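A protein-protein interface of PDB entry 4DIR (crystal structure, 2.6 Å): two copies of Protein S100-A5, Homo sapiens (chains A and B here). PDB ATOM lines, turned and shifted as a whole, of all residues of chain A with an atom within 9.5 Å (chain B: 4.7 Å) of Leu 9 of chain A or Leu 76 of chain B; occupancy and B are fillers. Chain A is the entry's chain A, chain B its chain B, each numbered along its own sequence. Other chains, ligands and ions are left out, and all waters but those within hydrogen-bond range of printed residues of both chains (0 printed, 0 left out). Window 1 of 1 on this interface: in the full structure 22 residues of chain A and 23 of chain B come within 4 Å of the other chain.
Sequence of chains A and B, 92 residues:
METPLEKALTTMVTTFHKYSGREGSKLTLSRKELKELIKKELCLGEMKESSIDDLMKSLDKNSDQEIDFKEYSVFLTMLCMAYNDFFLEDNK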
ATOM      1  N   THR A   3      30.641 -41.579   8.383  1.00  0.00           N
ATOM      2  CA  THR A   3      31.261 -40.482   7.678  1.00  0.00           C
ATOM      3  C   THR A   3      31.810 -39.549   8.692  1.00  0.00           C
ATOM      4  O   THR A   3      31.073 -38.875   9.362  1.00  0.00           O
ATOM      5  CB  THR A   3      30.239 -39.696   6.882  1.00  0.00           C
ATOM      6  N   PRO A   4      33.111 -39.487   8.814  1.00  0.00           N
ATOM      7  CA  PRO A   4      33.709 -38.604   9.800  1.00  0.00           C
ATOM      8  C   PRO A   4      32.958 -37.297   9.964  1.00  0.00           C
ATOM      9  O   PRO A   4      32.733 -36.880  11.078  1.00  0.00           O
ATOM     10  CB  PRO A   4      35.094 -38.381   9.231  1.00  0.00           C
ATOM     11  CG  PRO A   4      35.398 -39.650   8.596  1.00  0.00           C
ATOM     12  CD  PRO A   4      34.136 -40.075   7.947  1.00  0.00           C
ATOM     13  N   LEU A   5      32.555 -36.653   8.892  1.00  0.00           N
ATOM     14  CA  LEU A   5      31.811 -35.431   9.063  1.00  0.00           C
ATOM     15  C   LEU A   5      30.748 -35.664  10.097  1.00  0.00           C
ATOM     16  O   LEU A   5      30.591 -34.906  11.018  1.00  0.00           O
ATOM     17  CB  LEU A   5      31.165 -35.003   7.767  1.00  0.00           C
ATOM     18  CG  LEU A   5      31.214 -33.514   7.508  1.00  0.00           C
ATOM     19  CD1 LEU A   5      30.150 -33.064   6.619  1.00  0.00           C
ATOM     20  CD2 LEU A   5      31.141 -32.800   8.775  1.00  0.00           C
ATOM     21  N   GLU A   6      30.015 -36.745   9.925  1.00  0.00           N
ATOM     22  CA  GLU A   6      28.890 -37.075  10.762  1.00  0.00           C
ATOM     23  C   GLU A   6      29.311 -37.344  12.170  1.00  0.00           C
ATOM     24  O   GLU A   6      28.645 -36.980  13.095  1.00  0.00           O
ATOM     25  CB  GLU A   6      28.243 -38.327  10.236  1.00  0.00           C
ATOM     26  CG  GLU A   6      27.257 -38.109   9.160  1.00  0.00           C
ATOM     27  CD  GLU A   6      27.024 -39.360   8.370  1.00  0.00           C
ATOM     28  N   LYS A   7      30.412 -38.039  12.321  1.00  0.00           N
ATOM     29  CA  LYS A   7      30.969 -38.320  13.625  1.00  0.00           C
ATOM     30  C   LYS A   7      31.414 -37.001  14.269  1.00  0.00           C
ATOM     31  O   LYS A   7      31.293 -36.819  15.491  1.00  0.00           O
ATOM     32  CB  LYS A   7      32.109 -39.336  13.506  1.00  0.00           C
ATOM     33  N   ALA A   8      31.883 -36.059  13.441  1.00  0.00           N
ATOM     34  CA  ALA A   8      32.252 -34.726  13.928  1.00  0.00           C
ATOM     35  C   ALA A   8      31.060 -33.965  14.430  1.00  0.00           C
ATOM     36  O   ALA A   8      31.092 -33.439  15.541  1.00  0.00           O
ATOM     37  CB  ALA A   8      32.940 -33.942  12.860  1.00  0.00           C
ATOM     38  N   LEU A   9      30.016 -33.866  13.625  1.00  0.00           N
ATOM     39  CA  LEU A   9      28.803 -33.227  14.087  1.00  0.00           C
ATOM     40  C   LEU A   9      28.278 -33.851  15.372  1.00  0.00           C
ATOM     41  O   LEU A   9      27.815 -33.149  16.241  1.00  0.00           O
ATOM     42  CB  LEU A   9      27.742 -33.325  13.029  1.00  0.00           C
ATOM     43  CG  LEU A   9      28.206 -32.623  11.789  1.00  0.00           C
ATOM     44  CD1 LEU A   9      27.603 -33.280  10.600  1.00  0.00           C
ATOM     45  CD2 LEU A   9      27.801 -31.185  11.923  1.00  0.00           C
ATOM     46  N   THR A  10      28.365 -35.173  15.478  1.00  0.00           N
ATOM     47  CA  THR A  10      27.991 -35.896  16.669  1.00  0.00           C
ATOM     48  C   THR A  10      28.762 -35.385  17.870  1.00  0.00           C
ATOM     49  O   THR A  10      28.180 -35.146  18.905  1.00  0.00           O
ATOM     50  CB  THR A  10      28.161 -37.439  16.448  1.00  0.00           C
ATOM     51  OG1 THR A  10      27.230 -37.879  15.444  1.00  0.00           O
ATOM     52  CG2 THR A  10      27.966 -38.256  17.742  1.00  0.00           C
ATOM     53  N   THR A  11      30.075 -35.225  17.747  1.00  0.00           N
ATOM     54  CA  THR A  11      30.900 -34.730  18.845  1.00  0.00           C
ATOM     55  C   THR A  11      30.501 -33.334  19.295  1.00  0.00           C
ATOM     56  O   THR A  11      30.597 -33.021  20.491  1.00  0.00           O
ATOM     57  CB  THR A  11      32.347 -34.674  18.457  1.00  0.00           C
ATOM     58  OG1 THR A  11      32.761 -35.974  18.057  1.00  0.00           O
ATOM     59  CG2 THR A  11      33.191 -34.254  19.638  1.00  0.00           C
ATOM     60  N   MET A  12      30.073 -32.534  18.356  1.00  0.00           N
ATOM     61  CA  MET A  12      29.607 -31.232  18.639  1.00  0.00           C
ATOM     62  C   MET A  12      28.459 -31.231  19.626  1.00  0.00           C
ATOM     63  O   MET A  12      28.505 -30.527  20.585  1.00  0.00           O
ATOM     64  CB  MET A  12      29.181 -30.612  17.342  1.00  0.00           C
ATOM     65  CG  MET A  12      29.915 -29.387  17.021  1.00  0.00           C
ATOM     66  SD  MET A  12      31.469 -29.690  16.247  1.00  0.00           S
ATOM     67  CE  MET A  12      32.433 -30.002  17.683  1.00  0.00           C
ATOM     68  N   VAL A  13      27.426 -32.019  19.396  1.00  0.00           N
ATOM     69  CA  VAL A  13      26.227 -31.929  20.205  1.00  0.00           C
ATOM     70  C   VAL A  13      26.432 -32.650  21.510  1.00  0.00           C
ATOM     71  O   VAL A  13      26.137 -32.077  22.546  1.00  0.00           O
ATOM     72  CB  VAL A  13      24.856 -32.202  19.520  1.00  0.00           C
ATOM     73  CG1 VAL A  13      24.868 -31.906  18.023  1.00  0.00           C
ATOM     74  CG2 VAL A  13      24.413 -33.541  19.758  1.00  0.00           C
ATOM     75  N   THR A  14      27.034 -33.833  21.502  1.00  0.00           N
ATOM     76  CA  THR A  14      27.213 -34.567  22.761  1.00  0.00           C
ATOM     77  C   THR A  14      28.136 -33.850  23.753  1.00  0.00           C
ATOM     78  O   THR A  14      27.941 -33.909  24.969  1.00  0.00           O
ATOM     79  CB  THR A  14      27.764 -35.979  22.568  1.00  0.00           C
ATOM     80  OG1 THR A  14      29.171 -35.911  22.323  1.00  0.00           O
ATOM     81  CG2 THR A  14      27.060 -36.724  21.420  1.00  0.00           C
ATOM     82  N   THR A  15      29.146 -33.163  23.239  1.00  0.00           N
ATOM     83  CA  THR A  15      30.045 -32.386  24.082  1.00  0.00           C
ATOM     84  C   THR A  15      29.235 -31.299  24.776  1.00  0.00           C
ATOM     85  O   THR A  15      29.391 -31.068  25.949  1.00  0.00           O
ATOM     86  CB  THR A  15      31.207 -31.784  23.259  1.00  0.00           C
ATOM     87  OG1 THR A  15      32.048 -32.846  22.787  1.00  0.00           O
ATOM     88  CG2 THR A  15      32.051 -30.930  24.113  1.00  0.00           C
ATOM     89  N   PHE A  16      28.341 -30.649  24.047  1.00  0.00           N
ATOM     90  CA  PHE A  16      27.537 -29.602  24.653  1.00  0.00           C
ATOM     91  C   PHE A  16      26.836 -30.192  25.840  1.00  0.00           C
ATOM     92  O   PHE A  16      26.956 -29.678  26.950  1.00  0.00           O
ATOM     93  CB  PHE A  16      26.479 -29.084  23.699  1.00  0.00           C
ATOM     94  CG  PHE A  16      25.556 -28.064  24.320  1.00  0.00           C
ATOM     95  CD1 PHE A  16      25.957 -26.714  24.430  1.00  0.00           C
ATOM     96  CD2 PHE A  16      24.294 -28.428  24.769  1.00  0.00           C
ATOM     97  CE1 PHE A  16      25.118 -25.741  24.960  1.00  0.00           C
ATOM     98  CE2 PHE A  16      23.411 -27.465  25.322  1.00  0.00           C
ATOM     99  CZ  PHE A  16      23.816 -26.115  25.416  1.00  0.00           C
ATOM    100  N   HIS A  17      26.101 -31.278  25.596  1.00  0.00           N
ATOM    101  CA  HIS A  17      25.275 -31.919  26.615  1.00  0.00           C
ATOM    102  C   HIS A  17      26.110 -32.629  27.674  1.00  0.00           C
ATOM    103  O   HIS A  17      25.631 -32.757  28.800  1.00  0.00           O
ATOM    104  CB  HIS A  17      24.216 -32.833  25.994  1.00  0.00           C
ATOM    105  CG  HIS A  17      23.178 -32.087  25.209  1.00  0.00           C
ATOM    106  ND1 HIS A  17      23.199 -32.011  23.834  1.00  0.00           N
ATOM    107  CD2 HIS A  17      22.105 -31.360  25.606  1.00  0.00           C
ATOM    108  CE1 HIS A  17      22.177 -31.281  23.415  1.00  0.00           C
ATOM    109  NE2 HIS A  17      21.503 -30.869  24.473  1.00  0.00           N
ATOM    110  N   PHE A  69      21.999 -23.702  23.258  1.00  0.00           N
ATOM    111  CA  PHE A  69      22.670 -24.470  22.213  1.00  0.00           C
ATOM    112  C   PHE A  69      22.968 -23.649  20.960  1.00  0.00           C
ATOM    113  O   PHE A  69      24.043 -23.797  20.373  1.00  0.00           O
ATOM    114  CB  PHE A  69      21.919 -25.762  21.864  1.00  0.00           C
ATOM    115  CG  PHE A  69      22.681 -26.622  20.911  1.00  0.00           C
ATOM    116  CD1 PHE A  69      23.692 -27.465  21.366  1.00  0.00           C
ATOM    117  CD2 PHE A  69      22.467 -26.521  19.557  1.00  0.00           C
ATOM    118  CE1 PHE A  69      24.489 -28.244  20.460  1.00  0.00           C
ATOM    119  CE2 PHE A  69      23.255 -27.299  18.612  1.00  0.00           C
ATOM    120  CZ  PHE A  69      24.268 -28.161  19.066  1.00  0.00           C
ATOM    121  N   TYR A  72      25.973 -21.561  21.638  1.00  0.00           N
ATOM    122  CA  TYR A  72      27.153 -22.404  21.612  1.00  0.00           C
ATOM    123  C   TYR A  72      27.516 -22.584  20.155  1.00  0.00           C
ATOM    124  O   TYR A  72      28.693 -22.440  19.812  1.00  0.00           O
ATOM    125  CB  TYR A  72      26.845 -23.759  22.298  1.00  0.00           C
ATOM    126  CG  TYR A  72      27.789 -24.919  22.100  1.00  0.00           C
ATOM    127  CD1 TYR A  72      29.070 -24.972  22.707  1.00  0.00           C
ATOM    128  CD2 TYR A  72      27.361 -26.008  21.371  1.00  0.00           C
ATOM    129  CE1 TYR A  72      29.922 -26.130  22.537  1.00  0.00           C
ATOM    130  CE2 TYR A  72      28.165 -27.154  21.203  1.00  0.00           C
ATOM    131  CZ  TYR A  72      29.433 -27.222  21.772  1.00  0.00           C
ATOM    132  OH  TYR A  72      30.137 -28.411  21.489  1.00  0.00           O
ATOM    133  N   SER A  73      26.528 -22.739  19.310  1.00  0.00           N
ATOM    134  CA  SER A  73      26.723 -22.827  17.887  1.00  0.00           C
ATOM    135  C   SER A  73      27.593 -21.766  17.274  1.00  0.00           C
ATOM    136  O   SER A  73      28.294 -22.001  16.327  1.00  0.00           O
ATOM    137  CB  SER A  73      25.383 -22.743  17.225  1.00  0.00           C
ATOM    138  OG  SER A  73      25.086 -23.990  16.689  1.00  0.00           O
ATOM    139  N   LEU A  76      31.147 -22.599  18.111  1.00  0.00           N
ATOM    140  CA  LEU A  76      31.706 -23.618  17.231  1.00  0.00           C
ATOM    141  C   LEU A  76      32.163 -22.995  15.887  1.00  0.00           C
ATOM    142  O   LEU A  76      33.272 -23.285  15.402  1.00  0.00           O
ATOM    143  CB  LEU A  76      30.665 -24.705  17.002  1.00  0.00           C
ATOM    144  CG  LEU A  76      30.315 -25.497  18.245  1.00  0.00           C
ATOM    145  CD1 LEU A  76      29.322 -26.538  17.805  1.00  0.00           C
ATOM    146  CD2 LEU A  76      31.520 -26.139  18.863  1.00  0.00           C
ATOM    147  N   THR A  77      31.323 -22.114  15.324  1.00  0.00           N
ATOM    148  CA  THR A  77      31.662 -21.333  14.137  1.00  0.00           C
ATOM    149  C   THR A  77      32.944 -20.512  14.299  1.00  0.00           C
ATOM    150  O   THR A  77      33.815 -20.547  13.418  1.00  0.00           O
ATOM    151  CB  THR A  77      30.498 -20.401  13.744  1.00  0.00           C
ATOM    152  OG1 THR A  77      29.328 -21.203  13.547  1.00  0.00           O
ATOM    153  CG2 THR A  77      30.790 -19.644  12.495  1.00  0.00           C
ATOM    154  N   CYS A  80      35.715 -22.903  14.017  1.00  0.00           N
ATOM    155  CA  CYS A  80      35.988 -23.335  12.624  1.00  0.00           C
ATOM    156  C   CYS A  80      36.610 -22.223  11.788  1.00  0.00           C
ATOM    157  O   CYS A  80      37.543 -22.470  11.064  1.00  0.00           O
ATOM    158  CB  CYS A  80      34.736 -23.829  11.937  1.00  0.00           C
ATOM    159  SG  CYS A  80      34.180 -25.271  12.733  1.00  0.00           S
ATOM    160  N   MET A  81      36.103 -21.006  11.880  1.00  0.00           N
ATOM    161  CA  MET A  81      36.729 -19.929  11.146  1.00  0.00           C
ATOM    162  C   MET A  81      38.218 -19.879  11.462  1.00  0.00           C
ATOM    163  O   MET A  81      39.038 -19.614  10.590  1.00  0.00           O
ATOM    164  CB  MET A  81      36.132 -18.585  11.509  1.00  0.00           C
ATOM    165  CG  MET A  81      34.637 -18.507  11.414  1.00  0.00           C
ATOM    166  SD  MET A  81      33.958 -18.828   9.776  1.00  0.00           S
ATOM    167  CE  MET A  81      35.322 -18.432   8.677  1.00  0.00           C
ATOM    168  N   LEU B  42      27.915 -37.448   4.309  1.00  0.00           N
ATOM    169  CA  LEU B  42      26.699 -37.383   5.090  1.00  0.00           C
ATOM    170  C   LEU B  42      25.650 -38.240   4.390  1.00  0.00           C
ATOM    171  O   LEU B  42      25.450 -38.127   3.182  1.00  0.00           O
ATOM    172  CB  LEU B  42      26.187 -35.958   5.091  1.00  0.00           C
ATOM    173  CG  LEU B  42      26.858 -34.792   5.779  1.00  0.00           C
ATOM    174  CD1 LEU B  42      26.130 -33.557   5.294  1.00  0.00           C
ATOM    175  CD2 LEU B  42      26.704 -34.951   7.260  1.00  0.00           C
ATOM    176  N   TYR B  72      29.364 -22.490   4.130  1.00  0.00           N
ATOM    177  CA  TYR B  72      29.388 -23.879   4.554  1.00  0.00           C
ATOM    178  C   TYR B  72      29.228 -23.973   6.039  1.00  0.00           C
ATOM    179  O   TYR B  72      28.535 -24.849   6.529  1.00  0.00           O
ATOM    180  CB  TYR B  72      30.700 -24.468   4.133  1.00  0.00           C
ATOM    181  CG  TYR B  72      31.115 -25.834   4.679  1.00  0.00           C
ATOM    182  CD1 TYR B  72      30.577 -27.048   4.189  1.00  0.00           C
ATOM    183  CD2 TYR B  72      32.177 -25.911   5.599  1.00  0.00           C
ATOM    184  CE1 TYR B  72      31.071 -28.309   4.682  1.00  0.00           C
ATOM    185  CE2 TYR B  72      32.674 -27.127   6.083  1.00  0.00           C
ATOM    186  CZ  TYR B  72      32.128 -28.303   5.647  1.00  0.00           C
ATOM    187  OH  TYR B  72      32.694 -29.435   6.196  1.00  0.00           O
ATOM    188  N   SER B  73      29.838 -23.037   6.763  1.00  0.00           N
ATOM    189  CA  SER B  73      29.723 -22.936   8.231  1.00  0.00           C
ATOM    190  C   SER B  73      28.299 -22.894   8.654  1.00  0.00           C
ATOM    191  O   SER B  73      27.964 -23.500   9.648  1.00  0.00           O
ATOM    192  CB  SER B  73      30.429 -21.678   8.775  1.00  0.00           C
ATOM    193  N   VAL B  74      27.454 -22.209   7.891  1.00  0.00           N
ATOM    194  CA  VAL B  74      26.030 -22.139   8.201  1.00  0.00           C
ATOM    195  C   VAL B  74      25.343 -23.489   8.002  1.00  0.00           C
ATOM    196  O   VAL B  74      24.372 -23.808   8.688  1.00  0.00           O
ATOM    197  CB  VAL B  74      25.317 -21.080   7.339  1.00  0.00           C
ATOM    198  CG1 VAL B  74      23.809 -21.187   7.508  1.00  0.00           C
ATOM    199  CG2 VAL B  74      25.804 -19.685   7.702  1.00  0.00           C
ATOM    200  N   PHE B  75      25.853 -24.277   7.059  1.00  0.00           N
ATOM    201  CA  PHE B  75      25.284 -25.587   6.758  1.00  0.00           C
ATOM    202  C   PHE B  75      25.598 -26.407   7.975  1.00  0.00           C
ATOM    203  O   PHE B  75      24.677 -26.902   8.619  1.00  0.00           O
ATOM    204  CB  PHE B  75      25.905 -26.152   5.452  1.00  0.00           C
ATOM    205  CG  PHE B  75      25.416 -27.525   5.053  1.00  0.00           C
ATOM    206  CD1 PHE B  75      24.070 -27.887   5.200  1.00  0.00           C
ATOM    207  CD2 PHE B  75      26.306 -28.452   4.482  1.00  0.00           C
ATOM    208  CE1 PHE B  75      23.626 -29.127   4.832  1.00  0.00           C
ATOM    209  CE2 PHE B  75      25.854 -29.719   4.084  1.00  0.00           C
ATOM    210  CZ  PHE B  75      24.509 -30.046   4.264  1.00  0.00           C
ATOM    211  N   LEU B  76      26.877 -26.475   8.343  1.00  0.00           N
ATOM    212  CA  LEU B  76      27.281 -27.221   9.536  1.00  0.00           C
ATOM    213  C   LEU B  76      26.410 -26.920  10.778  1.00  0.00           C
ATOM    214  O   LEU B  76      25.970 -27.857  11.453  1.00  0.00           O
ATOM    215  CB  LEU B  76      28.750 -26.975   9.842  1.00  0.00           C
ATOM    216  CG  LEU B  76      29.845 -27.429   8.855  1.00  0.00           C
ATOM    217  CD2 LEU B  76      29.616 -28.851   8.432  1.00  0.00           C
ATOM    218  N   THR B  77      26.109 -25.634  11.039  1.00  0.00           N
ATOM    219  CA  THR B  77      25.161 -25.211  12.114  1.00  0.00           C
ATOM    220  C   THR B  77      23.774 -25.836  12.024  1.00  0.00           C
ATOM    221  O   THR B  77      23.279 -26.436  12.994  1.00  0.00           O
ATOM    222  CB  THR B  77      25.014 -23.650  12.174  1.00  0.00           C
ATOM    223  OG1 THR B  77      26.290 -23.028  12.316  1.00  0.00           O
ATOM    224  CG2 THR B  77      24.176 -23.203  13.353  1.00  0.00           C
ATOM    225  N   MET B  78      23.128 -25.675  10.871  1.00  0.00           N
ATOM    226  CA  MET B  78      21.820 -26.300  10.639  1.00  0.00           C
ATOM    227  C   MET B  78      21.919 -27.752  11.028  1.00  0.00           C
ATOM    228  O   MET B  78      21.082 -28.215  11.754  1.00  0.00           O
ATOM    229  CB  MET B  78      21.391 -26.175   9.180  1.00  0.00           C
ATOM    230  N   LEU B  79      22.964 -28.454  10.573  1.00  0.00           N
ATOM    231  CA  LEU B  79      23.167 -29.878  10.938  1.00  0.00           C
ATOM    232  C   LEU B  79      23.223 -30.105  12.458  1.00  0.00           C
ATOM    233  O   LEU B  79      22.548 -30.993  12.975  1.00  0.00           O
ATOM    234  CB  LEU B  79      24.429 -30.465  10.253  1.00  0.00           C
ATOM    235  CG  LEU B  79      24.431 -30.669   8.727  1.00  0.00           C
ATOM    236  CD1 LEU B  79      25.748 -31.233   8.243  1.00  0.00           C
ATOM    237  CD2 LEU B  79      23.297 -31.605   8.294  1.00  0.00           C
ATOM    238  N   CYS B  80      24.020 -29.291  13.152  1.00  0.00           N
ATOM    239  CA  CYS B  80      24.163 -29.417  14.580  1.00  0.00           C
ATOM    240  C   CYS B  80      22.850 -29.190  15.278  1.00  0.00           C
ATOM    241  O   CYS B  80      22.490 -29.950  16.154  1.00  0.00           O
ATOM    242  CB  CYS B  80      25.230 -28.471  15.109  1.00  0.00           C
ATOM    243  SG  CYS B  80      26.912 -29.070  14.738  1.00  0.00           S
ATOM    244  N   TYR B  83      21.065 -32.414  14.659  1.00  0.00           N
ATOM    245  CA  TYR B  83      21.633 -33.463  15.448  1.00  0.00           C
ATOM    246  C   TYR B  83      21.285 -33.246  16.905  1.00  0.00           C
ATOM    247  O   TYR B  83      21.230 -34.175  17.669  1.00  0.00           O
ATOM    248  CB  TYR B  83      23.135 -33.493  15.257  1.00  0.00           C
ATOM    249  CG  TYR B  83      23.560 -34.203  14.016  1.00  0.00           C
ATOM    250  CD1 TYR B  83      23.089 -33.812  12.793  1.00  0.00           C
ATOM    251  CD2 TYR B  83      24.411 -35.273  14.069  1.00  0.00           C
ATOM    252  CE1 TYR B  83      23.457 -34.454  11.665  1.00  0.00           C
ATOM    253  CE2 TYR B  83      24.778 -35.924  12.942  1.00  0.00           C
ATOM    254  CZ  TYR B  83      24.294 -35.505  11.744  1.00  0.00           C
ATOM    255  OH  TYR B  83      24.651 -36.137  10.601  1.00  0.00           O
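The backbone carbonyl oxygen of Glu 6 of chain A lies within hydrogen-bond range of the side-chain hydroxyl of Thr 10 of chain A. The backbone carbonyl oxygen (O) of Val 13 of chain A is in hydrogen-bond range of a ring nitrogen (ND1) of His 17 of chain A, 3.2 Å away. The backbone carbonyl oxygen (O) of Ser 73 of chain A lies within hydrogen-bond range of the side-chain hydroxyl (OG1) of Thr 77 of chain A (3.1 Å). O of Met 12 of chain A sits at hydrogen-bond distance from OH of Tyr 72 of chain A, 2.8 Å away. OG1 of Thr 77 of chain B lies within hydrogen-bond range of O of Ser 73 of chain B (3.2 Å). O of Leu 76 of chain B is in hydrogen-bond range of SG of Cys 80 of chain B.
Glu 6 of chain A touches Leu 42 of chain B (CG to CD2, 3.7 Å). CG of Glu 6 of chain A touches OH of Tyr 83 of chain B, at 3.6 Å. Leu 42 of chain B touches Leu 9 of chain A. Leu 76 of chain B touches Leu 9 of chain A. Cys 80 of chain B touches Leu 9 of chain A. Leu 9 of chain A touches Tyr 83 of chain B. O of Cys 80 of chain B touches CG1 of Val 13 of chain A, 3.6 Å away. Val 13 of chain A touches Tyr 83 of chain B (CG1 to CB, 3.6 Å). Cys 80 of chain B touches Phe 69 of chain A. OG of Ser 73 of chain A touches CG2 of Thr 77 of chain B, at 3.5 Å.
Of the printed residues of chain B, Leu 5 of chain A touches Leu 42. Lys 7 of chain A touches none of the printed residues of chain B. Leu 9 of chain A touches five residues of chain B. Of the printed residues of chain B, Met 12 of chain A touches Cys 80 (3.8 Å). Of the printed residues of chain B, Ser 73 of chain A touches Thr 77. Of the printed residues of chain A, Leu 42 of chain B touches Leu 5 (3.8 Å), Glu 6 (3.7 Å) and Leu 9 (3.8 Å). Leu 76 of chain B touches just one residue of chain A: Leu 9. No residue of chain A comes within 4 Å of Met 78 of chain B. Of chain A, only Leu 9 (3.6 Å) comes within 4 Å of Leu 79 of chain B. Of the printed residues of chain A, Tyr 83 of chain B touches Glu 6, Leu 9 and Val 13. The nearest printed residue of chain B that does not touch Leu 9 of chain A is Thr 77 of chain B (5.9 Å). The nearest printed residue of chain B that does not touch Met 12 of chain A is Leu 76 of chain B (7.0 Å).
Hydrophobic or aromatic side chains of chain B within 4 Å of the printed part of chain A: Leu 42, Leu 79 and Tyr 83. Hydrophobic or aromatic side chains of chain A within 4 Å of the printed part of chain B: Leu 5, Leu 9, Met 12, Val 13 and Phe 69. Among the printed residues, 14 pairs touch across the chains. Among the printed residues, no Asp or Glu carboxylate lies within 4 Å of a Lys or Arg side-chain nitrogen of the other chain.
Ser 73 of chain A touches Thr 77 of chain B, but with the chains exchanged Thr 77 of chain A does not touch Ser 73 of chain B (4.3 Å). Thr 77 of chain A touches its own counterpart, Thr 77 of chain B. Positions printed for both chains: 72, 73, 76, 77 and 80. Of the 14 pairs that touch across the chains among the printed residues, 1 has its exchanged pair printed and touching as well.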
